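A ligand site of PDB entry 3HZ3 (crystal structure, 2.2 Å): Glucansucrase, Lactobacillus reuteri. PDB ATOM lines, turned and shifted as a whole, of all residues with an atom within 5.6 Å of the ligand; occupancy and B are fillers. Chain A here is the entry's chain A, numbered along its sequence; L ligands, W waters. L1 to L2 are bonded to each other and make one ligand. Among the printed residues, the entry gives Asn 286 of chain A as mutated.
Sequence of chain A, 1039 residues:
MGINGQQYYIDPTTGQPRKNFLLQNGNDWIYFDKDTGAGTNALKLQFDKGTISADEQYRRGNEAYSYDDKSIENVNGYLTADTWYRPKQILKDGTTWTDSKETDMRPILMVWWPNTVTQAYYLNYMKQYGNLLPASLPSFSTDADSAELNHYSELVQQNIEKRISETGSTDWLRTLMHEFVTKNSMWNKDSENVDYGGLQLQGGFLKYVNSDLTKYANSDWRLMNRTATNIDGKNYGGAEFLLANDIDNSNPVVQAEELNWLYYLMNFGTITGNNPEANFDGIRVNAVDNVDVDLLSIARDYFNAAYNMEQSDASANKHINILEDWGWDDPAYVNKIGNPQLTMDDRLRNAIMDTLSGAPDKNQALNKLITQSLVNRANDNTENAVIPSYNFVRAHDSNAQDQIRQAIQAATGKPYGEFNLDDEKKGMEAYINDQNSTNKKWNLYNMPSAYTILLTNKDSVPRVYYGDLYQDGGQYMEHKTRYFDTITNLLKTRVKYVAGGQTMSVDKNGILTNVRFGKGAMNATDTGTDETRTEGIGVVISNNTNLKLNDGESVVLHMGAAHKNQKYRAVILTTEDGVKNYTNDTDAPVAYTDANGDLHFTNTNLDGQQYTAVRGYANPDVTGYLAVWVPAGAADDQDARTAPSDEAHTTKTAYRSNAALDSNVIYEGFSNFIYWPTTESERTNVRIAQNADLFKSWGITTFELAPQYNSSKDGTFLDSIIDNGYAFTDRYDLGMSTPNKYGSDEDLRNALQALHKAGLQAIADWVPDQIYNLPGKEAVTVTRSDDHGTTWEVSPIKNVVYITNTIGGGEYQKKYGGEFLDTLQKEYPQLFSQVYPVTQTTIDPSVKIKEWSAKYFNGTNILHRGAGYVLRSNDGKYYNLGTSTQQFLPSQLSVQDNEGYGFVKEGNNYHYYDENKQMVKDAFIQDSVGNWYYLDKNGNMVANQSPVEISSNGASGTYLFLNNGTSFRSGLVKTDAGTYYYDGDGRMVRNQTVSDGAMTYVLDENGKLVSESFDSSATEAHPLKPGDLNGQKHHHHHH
An oxygen (O6) of LG2 L2 lies within hydrogen-bond range of the side-chain amide nitrogen (NE2) of Gln 401 (3.2 Å). An oxygen (O1) of LIG L1 is in hydrogen-bond range of the guanidinium group of Arg 284 (3.1 Å). The side-chain carboxylate (OE2) of Glu 324 sits at hydrogen-bond distance from an oxygen (O1) of LG2 L2 (2.9 Å). An oxygen (O3) of LIG L1 lies within hydrogen-bond range of the side-chain carboxylate (OD2) of Asp 719. The side-chain carboxylate (OD2) of Asp 397 is in hydrogen-bond range of an oxygen (O1) of LIG L1, at 2.8 Å. O3 of LG2 L2 sits at hydrogen-bond distance from NE1 of Trp 326 (3.4 Å). The side-chain amide nitrogen (NE2) of Gln 770 sits at hydrogen-bond distance from an oxygen (O5) of LIG L1, at 3.3 Å. The side-chain amide nitrogen (ND2) of Asn 286 sits at hydrogen-bond distance from an oxygen (O5) of LIG L1 (2.7 Å). NE2 of His 396 sits at hydrogen-bond distance from O2 of LIG L1.
ND2 of Asn 672 lies within hydrogen-bond range of OE1 of Gln 401, at 2.9 Å. N of Ala 287 lies within hydrogen-bond range of OE1 of Glu 324 (2.8 Å). OD1 of Asn 286 sits close to OE1 of Glu 324, at 2.9 Å. OE1 of Gln 770 lies close to OD1 of Asp 769. The guanidinium group (NH1) of Arg 284 is in hydrogen-bond range of the side-chain hydroxyl (OH) of Tyr 726 (3.1 Å). OD1 of Asn 286 is in hydrogen-bond range of NH1 of Arg 284 (3.2 Å). OE1 of Glu 324 lies within salt-bridge range of NH2 of Arg 284, at 3.2 Å. A ring nitrogen (NE2) of His 396 lies close to the side-chain hydroxyl (OH) of Tyr 726, at 3.5 Å.
Merely in contact with the ligand: Leu 201 (3.6 Å), Leu 242 (3.7 Å), Leu 243 (3.7 Å), Phe 717 (3.6 Å) and Tyr 726 (3.2 Å). Hydrophobic or aromatic side chains that line the ligand: Leu 201, Leu 242, Leu 243, Trp 326, His 396, Phe 717 and Tyr 726. 14 residues have an atom within 4 Å of the ligand: Leu 201, Leu 242, Leu 243, Arg 284, Asn 286, Glu 324, Trp 326, His 396, Asp 397, Gln 401, Phe 717, Asp 719, Tyr 726 and Gln 770.
Water W1 lies within hydrogen-bond range of O2 of LIG L1 (2.6 Å), OE1 of Gln 401 (2.7 Å), OD1 of Asp 719 (2.7 Å), ND2 of Asn 672 (3.2 Å) and ND2 of Asn 724 (3.3 Å). Water W3 bridges the side-chain amide oxygen (OD1) of Asn 290 (2.6 Å) and an oxygen (O1) of LG2 L2 (2.7 Å).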
ATOM      1  N   LEU A 201      25.589   7.156 -20.848  1.00  0.00           N
ATOM      2  CA  LEU A 201      25.762   8.484 -21.448  1.00  0.00           C
ATOM      3  C   LEU A 201      26.692   9.258 -20.562  1.00  0.00           C
ATOM      4  O   LEU A 201      27.358  10.171 -21.021  1.00  0.00           O
ATOM      5  CB  LEU A 201      24.416   9.218 -21.532  1.00  0.00           C
ATOM      6  CG  LEU A 201      23.359   8.622 -22.486  1.00  0.00           C
ATOM      7  CD1 LEU A 201      22.121   9.520 -22.551  1.00  0.00           C
ATOM      8  CD2 LEU A 201      23.931   8.410 -23.888  1.00  0.00           C
ATOM      9  N   LEU A 242      19.810   4.943 -18.023  1.00  0.00           N
ATOM     10  CA  LEU A 242      19.962   6.035 -19.008  1.00  0.00           C
ATOM     11  C   LEU A 242      20.757   7.223 -18.443  1.00  0.00           C
ATOM     12  O   LEU A 242      21.832   7.536 -18.942  1.00  0.00           O
ATOM     13  CB  LEU A 242      18.586   6.512 -19.557  1.00  0.00           C
ATOM     14  CG  LEU A 242      18.555   7.646 -20.613  1.00  0.00           C
ATOM     15  CD1 LEU A 242      19.325   7.297 -21.886  1.00  0.00           C
ATOM     16  CD2 LEU A 242      17.136   8.044 -21.000  1.00  0.00           C
ATOM     17  N   LEU A 243      20.230   7.885 -17.424  1.00  0.00           N
ATOM     18  CA  LEU A 243      20.830   9.093 -16.869  1.00  0.00           C
ATOM     19  C   LEU A 243      20.540   9.152 -15.378  1.00  0.00           C
ATOM     20  O   LEU A 243      19.438   8.763 -14.936  1.00  0.00           O
ATOM     21  CB  LEU A 243      20.231  10.352 -17.524  1.00  0.00           C
ATOM     22  CG  LEU A 243      20.619  10.622 -18.987  1.00  0.00           C
ATOM     23  CD1 LEU A 243      19.677  11.565 -19.614  1.00  0.00           C
ATOM     24  CD2 LEU A 243      22.111  11.105 -19.130  1.00  0.00           C
ATOM     25  N   ARG A 284       3.287  13.216 -23.396  1.00  0.00           N
ATOM     26  CA  ARG A 284       4.345  12.552 -24.107  1.00  0.00           C
ATOM     27  C   ARG A 284       4.952  11.618 -23.053  1.00  0.00           C
ATOM     28  O   ARG A 284       5.348  12.073 -21.961  1.00  0.00           O
ATOM     29  CB  ARG A 284       5.385  13.551 -24.634  1.00  0.00           C
ATOM     30  CG  ARG A 284       6.605  12.895 -25.269  1.00  0.00           C
ATOM     31  CD  ARG A 284       7.545  13.945 -25.780  1.00  0.00           C
ATOM     32  NE  ARG A 284       8.782  13.417 -26.348  1.00  0.00           N
ATOM     33  CZ  ARG A 284       9.911  13.258 -25.671  1.00  0.00           C
ATOM     34  NH1 ARG A 284       9.953  13.540 -24.377  1.00  0.00           N
ATOM     35  NH2 ARG A 284      10.990  12.797 -26.261  1.00  0.00           N
ATOM     36  N   ASN A 286       7.984  10.132 -22.133  1.00  0.00           N
ATOM     37  CA  ASN A 286       9.423  10.219 -22.376  1.00  0.00           C
ATOM     38  C   ASN A 286      10.169   8.917 -22.026  1.00  0.00           C
ATOM     39  O   ASN A 286       9.846   8.250 -21.040  1.00  0.00           O
ATOM     40  CB  ASN A 286       9.978  11.377 -21.545  1.00  0.00           C
ATOM     41  CG  ASN A 286      11.468  11.487 -21.616  1.00  0.00           C
ATOM     42  OD1 ASN A 286      12.029  11.753 -22.695  1.00  0.00           O
ATOM     43  ND2 ASN A 286      12.139  11.305 -20.479  1.00  0.00           N
ATOM     44  N   ALA A 287      11.170   8.575 -22.845  1.00  0.00           N
ATOM     45  CA  ALA A 287      12.091   7.454 -22.562  1.00  0.00           C
ATOM     46  C   ALA A 287      11.371   6.145 -22.263  1.00  0.00           C
ATOM     47  O   ALA A 287      11.657   5.458 -21.278  1.00  0.00           O
ATOM     48  CB  ALA A 287      13.051   7.818 -21.419  1.00  0.00           C
ATOM     49  N   ASN A 290      13.030   2.728 -21.625  1.00  0.00           N
ATOM     50  CA  ASN A 290      13.931   2.757 -20.472  1.00  0.00           C
ATOM     51  C   ASN A 290      13.226   2.566 -19.153  1.00  0.00           C
ATOM     52  O   ASN A 290      13.831   2.728 -18.087  1.00  0.00           O
ATOM     53  CB  ASN A 290      14.713   4.067 -20.474  1.00  0.00           C
ATOM     54  CG  ASN A 290      15.469   4.274 -21.759  1.00  0.00           C
ATOM     55  OD1 ASN A 290      15.210   5.237 -22.512  1.00  0.00           O
ATOM     56  ND2 ASN A 290      16.424   3.360 -22.045  1.00  0.00           N
ATOM     57  N   GLU A 324       7.438   8.430 -26.719  1.00  0.00           N
ATOM     58  CA  GLU A 324       8.812   8.391 -27.215  1.00  0.00           C
ATOM     59  C   GLU A 324       9.345   6.951 -27.161  1.00  0.00           C
ATOM     60  O   GLU A 324      10.137   6.602 -26.289  1.00  0.00           O
ATOM     61  CB  GLU A 324       9.740   9.368 -26.520  1.00  0.00           C
ATOM     62  CG  GLU A 324      11.102   9.421 -27.203  1.00  0.00           C
ATOM     63  CD  GLU A 324      12.195   9.922 -26.292  1.00  0.00           C
ATOM     64  OE1 GLU A 324      11.953  10.036 -25.067  1.00  0.00           O
ATOM     65  OE2 GLU A 324      13.273  10.228 -26.823  1.00  0.00           O
ATOM     66  N   TRP A 326      11.337   4.267 -29.263  1.00  0.00           N
ATOM     67  CA  TRP A 326      12.284   4.102 -30.348  1.00  0.00           C
ATOM     68  C   TRP A 326      12.379   2.685 -30.923  1.00  0.00           C
ATOM     69  O   TRP A 326      12.771   2.526 -32.087  1.00  0.00           O
ATOM     70  CB  TRP A 326      13.702   4.554 -29.875  1.00  0.00           C
ATOM     71  CG  TRP A 326      13.796   6.068 -29.575  1.00  0.00           C
ATOM     72  CD1 TRP A 326      13.877   6.681 -28.341  1.00  0.00           C
ATOM     73  CD2 TRP A 326      13.801   7.132 -30.546  1.00  0.00           C
ATOM     74  NE1 TRP A 326      13.943   8.056 -28.499  1.00  0.00           N
ATOM     75  CE2 TRP A 326      13.916   8.355 -29.838  1.00  0.00           C
ATOM     76  CE3 TRP A 326      13.741   7.165 -31.956  1.00  0.00           C
ATOM     77  CZ2 TRP A 326      13.980   9.604 -30.491  1.00  0.00           C
ATOM     78  CZ3 TRP A 326      13.754   8.418 -32.608  1.00  0.00           C
ATOM     79  CH2 TRP A 326      13.870   9.620 -31.877  1.00  0.00           C
ATOM     80  N   HIS A 396      13.975  18.004 -30.605  1.00  0.00           N
ATOM     81  CA  HIS A 396      14.944  18.708 -29.776  1.00  0.00           C
ATOM     82  C   HIS A 396      16.193  17.851 -29.596  1.00  0.00           C
ATOM     83  O   HIS A 396      17.301  18.376 -29.525  1.00  0.00           O
ATOM     84  CB  HIS A 396      14.333  19.052 -28.432  1.00  0.00           C
ATOM     85  CG  HIS A 396      14.068  17.844 -27.586  1.00  0.00           C
ATOM     86  ND1 HIS A 396      12.884  17.133 -27.651  1.00  0.00           N
ATOM     87  CD2 HIS A 396      14.861  17.172 -26.718  1.00  0.00           C
ATOM     88  CE1 HIS A 396      12.942  16.114 -26.817  1.00  0.00           C
ATOM     89  NE2 HIS A 396      14.128  16.107 -26.251  1.00  0.00           N
ATOM     90  N   ASP A 397      16.032  16.536 -29.547  1.00  0.00           N
ATOM     91  CA  ASP A 397      17.209  15.668 -29.456  1.00  0.00           C
ATOM     92  C   ASP A 397      17.609  15.101 -30.816  1.00  0.00           C
ATOM     93  O   ASP A 397      18.698  15.441 -31.369  1.00  0.00           O
ATOM     94  CB  ASP A 397      17.083  14.603 -28.318  1.00  0.00           C
ATOM     95  CG  ASP A 397      15.795  13.770 -28.427  1.00  0.00           C
ATOM     96  OD1 ASP A 397      14.990  14.013 -29.368  1.00  0.00           O
ATOM     97  OD2 ASP A 397      15.607  12.859 -27.576  1.00  0.00           O
ATOM     98  N   GLN A 401      20.584  17.921 -31.150  1.00  0.00           N
ATOM     99  CA  GLN A 401      21.507  18.145 -30.015  1.00  0.00           C
ATOM    100  C   GLN A 401      22.976  17.739 -30.274  1.00  0.00           C
ATOM    101  O   GLN A 401      23.873  18.440 -29.832  1.00  0.00           O
ATOM    102  CB  GLN A 401      20.959  17.601 -28.673  1.00  0.00           C
ATOM    103  CG  GLN A 401      20.971  16.076 -28.506  1.00  0.00           C
ATOM    104  CD  GLN A 401      20.266  15.637 -27.219  1.00  0.00           C
ATOM    105  OE1 GLN A 401      19.483  16.390 -26.664  1.00  0.00           O
ATOM    106  NE2 GLN A 401      20.547  14.395 -26.758  1.00  0.00           N
ATOM    107  N   ASN A 672      16.353  22.652 -27.421  1.00  0.00           N
ATOM    108  CA  ASN A 672      17.252  22.623 -26.271  1.00  0.00           C
ATOM    109  C   ASN A 672      17.955  23.945 -26.115  1.00  0.00           C
ATOM    110  O   ASN A 672      18.315  24.307 -25.009  1.00  0.00           O
ATOM    111  CB  ASN A 672      18.293  21.524 -26.427  1.00  0.00           C
ATOM    112  CG  ASN A 672      17.742  20.164 -26.116  1.00  0.00           C
ATOM    113  OD1 ASN A 672      16.569  20.011 -25.732  1.00  0.00           O
ATOM    114  ND2 ASN A 672      18.581  19.163 -26.285  1.00  0.00           N
ATOM    115  N   PHE A 717      24.701  16.750 -17.403  1.00  0.00           N
ATOM    116  CA  PHE A 717      24.256  16.341 -18.728  1.00  0.00           C
ATOM    117  C   PHE A 717      23.795  17.564 -19.534  1.00  0.00           C
ATOM    118  O   PHE A 717      23.475  18.623 -18.969  1.00  0.00           O
ATOM    119  CB  PHE A 717      23.173  15.255 -18.671  1.00  0.00           C
ATOM    120  CG  PHE A 717      22.856  14.673 -20.024  1.00  0.00           C
ATOM    121  CD1 PHE A 717      23.855  14.008 -20.764  1.00  0.00           C
ATOM    122  CD2 PHE A 717      21.595  14.812 -20.568  1.00  0.00           C
ATOM    123  CE1 PHE A 717      23.593  13.516 -22.030  1.00  0.00           C
ATOM    124  CE2 PHE A 717      21.311  14.319 -21.839  1.00  0.00           C
ATOM    125  CZ  PHE A 717      22.312  13.650 -22.565  1.00  0.00           C
ATOM    126  N   ASP A 719      21.068  18.283 -20.702  1.00  0.00           N
ATOM    127  CA  ASP A 719      19.781  18.791 -20.155  1.00  0.00           C
ATOM    128  C   ASP A 719      19.944  19.745 -18.977  1.00  0.00           C
ATOM    129  O   ASP A 719      19.108  20.628 -18.792  1.00  0.00           O
ATOM    130  CB  ASP A 719      18.854  17.647 -19.750  1.00  0.00           C
ATOM    131  CG  ASP A 719      18.502  16.708 -20.902  1.00  0.00           C
ATOM    132  OD1 ASP A 719      18.768  17.015 -22.089  1.00  0.00           O
ATOM    133  OD2 ASP A 719      17.946  15.650 -20.587  1.00  0.00           O
ATOM    134  N   ASN A 724      16.603  22.399 -20.227  1.00  0.00           N
ATOM    135  CA  ASN A 724      15.456  22.169 -21.091  1.00  0.00           C
ATOM    136  C   ASN A 724      14.215  21.705 -20.307  1.00  0.00           C
ATOM    137  O   ASN A 724      13.065  21.922 -20.739  1.00  0.00           O
ATOM    138  CB  ASN A 724      15.785  21.259 -22.291  1.00  0.00           C
ATOM    139  CG  ASN A 724      16.351  19.892 -21.898  1.00  0.00           C
ATOM    140  OD1 ASN A 724      16.275  19.514 -20.732  1.00  0.00           O
ATOM    141  ND2 ASN A 724      16.940  19.157 -22.897  1.00  0.00           N
ATOM    142  N   TYR A 726      14.330  18.416 -18.827  1.00  0.00           N
ATOM    143  CA  TYR A 726      14.401  16.967 -18.743  1.00  0.00           C
ATOM    144  C   TYR A 726      15.166  16.469 -17.524  1.00  0.00           C
ATOM    145  O   TYR A 726      14.991  15.345 -17.115  1.00  0.00           O
ATOM    146  CB  TYR A 726      14.994  16.348 -20.028  1.00  0.00           C
ATOM    147  CG  TYR A 726      14.034  16.324 -21.177  1.00  0.00           C
ATOM    148  CD1 TYR A 726      12.848  15.603 -21.096  1.00  0.00           C
ATOM    149  CD2 TYR A 726      14.267  17.089 -22.329  1.00  0.00           C
ATOM    150  CE1 TYR A 726      11.917  15.617 -22.133  1.00  0.00           C
ATOM    151  CE2 TYR A 726      13.353  17.083 -23.420  1.00  0.00           C
ATOM    152  CZ  TYR A 726      12.185  16.352 -23.291  1.00  0.00           C
ATOM    153  OH  TYR A 726      11.254  16.318 -24.291  1.00  0.00           O
ATOM    154  N   VAL A 767       8.023  12.555 -17.530  1.00  0.00           N
ATOM    155  CA  VAL A 767       9.432  12.089 -17.432  1.00  0.00           C
ATOM    156  C   VAL A 767       9.682  11.186 -16.179  1.00  0.00           C
ATOM    157  O   VAL A 767      10.432  11.574 -15.266  1.00  0.00           O
ATOM    158  CB  VAL A 767      10.366  13.316 -17.378  1.00  0.00           C
ATOM    159  CG1 VAL A 767      11.852  12.901 -17.402  1.00  0.00           C
ATOM    160  CG2 VAL A 767      10.070  14.284 -18.558  1.00  0.00           C
ATOM    161  N   ASP A 769      11.328   8.384 -15.902  1.00  0.00           N
ATOM    162  CA  ASP A 769      12.598   7.604 -15.888  1.00  0.00           C
ATOM    163  C   ASP A 769      13.533   7.906 -14.715  1.00  0.00           C
ATOM    164  O   ASP A 769      14.120   6.980 -14.164  1.00  0.00           O
ATOM    165  CB  ASP A 769      13.419   7.747 -17.157  1.00  0.00           C
ATOM    166  CG  ASP A 769      14.553   6.714 -17.223  1.00  0.00           C
ATOM    167  OD1 ASP A 769      15.750   7.102 -17.306  1.00  0.00           O
ATOM    168  OD2 ASP A 769      14.228   5.501 -17.156  1.00  0.00           O
ATOM    169  N   GLN A 770      13.720   9.173 -14.393  1.00  0.00           N
ATOM    170  CA  GLN A 770      14.862   9.580 -13.564  1.00  0.00           C
ATOM    171  C   GLN A 770      14.680  10.951 -12.914  1.00  0.00           C
ATOM    172  O   GLN A 770      13.697  11.653 -13.176  1.00  0.00           O
ATOM    173  CB  GLN A 770      16.183   9.547 -14.365  1.00  0.00           C
ATOM    174  CG  GLN A 770      16.451  10.798 -15.235  1.00  0.00           C
ATOM    175  CD  GLN A 770      15.756  10.780 -16.610  1.00  0.00           C
ATOM    176  OE1 GLN A 770      15.805   9.773 -17.320  1.00  0.00           O
ATOM    177  NE2 GLN A 770      15.129  11.909 -16.986  1.00  0.00           N
ATOM    178  N   TYR A 772      17.490  14.098 -10.952  1.00  0.00           N
ATOM    179  CA  TYR A 772      18.865  14.502 -10.839  1.00  0.00           C
ATOM    180  C   TYR A 772      19.147  15.198  -9.512  1.00  0.00           C
ATOM    181  O   TYR A 772      18.242  15.772  -8.883  1.00  0.00           O
ATOM    182  CB  TYR A 772      19.251  15.492 -11.958  1.00  0.00           C
ATOM    183  CG  TYR A 772      19.446  14.965 -13.394  1.00  0.00           C
ATOM    184  CD1 TYR A 772      20.670  15.122 -14.031  1.00  0.00           C
ATOM    185  CD2 TYR A 772      18.391  14.404 -14.120  1.00  0.00           C
ATOM    186  CE1 TYR A 772      20.873  14.715 -15.334  1.00  0.00           C
ATOM    187  CE2 TYR A 772      18.581  13.983 -15.470  1.00  0.00           C
ATOM    188  CZ  TYR A 772      19.808  14.147 -16.053  1.00  0.00           C
ATOM    189  OH  TYR A 772      20.009  13.778 -17.351  1.00  0.00           O
HETATM  190  C1  LIG L   1      14.761  11.396 -24.110  1.00  0.00           C
HETATM  191  C2  LIG L   1      14.531  12.933 -24.240  1.00  0.00           C
HETATM  192  C3  LIG L   1      15.884  13.616 -24.082  1.00  0.00           C
HETATM  193  C4  LIG L   1      16.392  13.404 -22.608  1.00  0.00           C
HETATM  194  C5  LIG L   1      16.324  11.931 -22.174  1.00  0.00           C
HETATM  195  C6  LIG L   1      16.135  11.837 -20.655  1.00  0.00           C
HETATM  196  O1  LIG L   1      13.906  13.356 -25.472  1.00  0.00           O
HETATM  197  O2  LIG L   1      15.699  15.023 -24.379  1.00  0.00           O
HETATM  198  O3  LIG L   1      17.736  13.912 -22.436  1.00  0.00           O
HETATM  199  O4  LIG L   1      15.136  11.191 -22.681  1.00  0.00           O
HETATM  200  O5  LIG L   1      14.724  12.061 -20.305  1.00  0.00           O
HETATM  201  C1  LG2 L   2      16.014   8.791 -24.452  1.00  0.00           C
HETATM  202  C2  LG2 L   2      16.700   9.991 -25.012  1.00  0.00           C
HETATM  203  C3  LG2 L   2      17.230   9.739 -26.428  1.00  0.00           C
HETATM  204  C4  LG2 L   2      18.399  10.657 -26.468  1.00  0.00           C
HETATM  205  C5  LG2 L   2      19.013  10.348 -25.093  1.00  0.00           C
HETATM  206  C6  LG2 L   2      19.849  11.465 -24.468  1.00  0.00           C
HETATM  207  O1  LG2 L   2      14.935   8.416 -25.259  1.00  0.00           O
HETATM  208  O2  LG2 L   2      15.841  11.157 -25.043  1.00  0.00           O
HETATM  209  O3  LG2 L   2      16.278  10.190 -27.363  1.00  0.00           O
HETATM  210  O4  LG2 L   2      19.235  10.155 -27.492  1.00  0.00           O
HETATM  211  O5  LG2 L   2      17.891  10.281 -24.241  1.00  0.00           O
HETATM  212  O6  LG2 L   2      19.111  12.689 -24.461  1.00  0.00           O
HETATM  213  O   HOH W   1      17.799  16.527 -24.609  1.00  0.00           O
HETATM  214  O   HOH W   2      20.572   7.944 -27.777  1.00  0.00           O
HETATM  215  O   HOH W   3      14.592   5.747 -25.028  1.00  0.00           O
HETATM  216  O   HOH W   4      19.974  12.393 -30.012  1.00  0.00           O
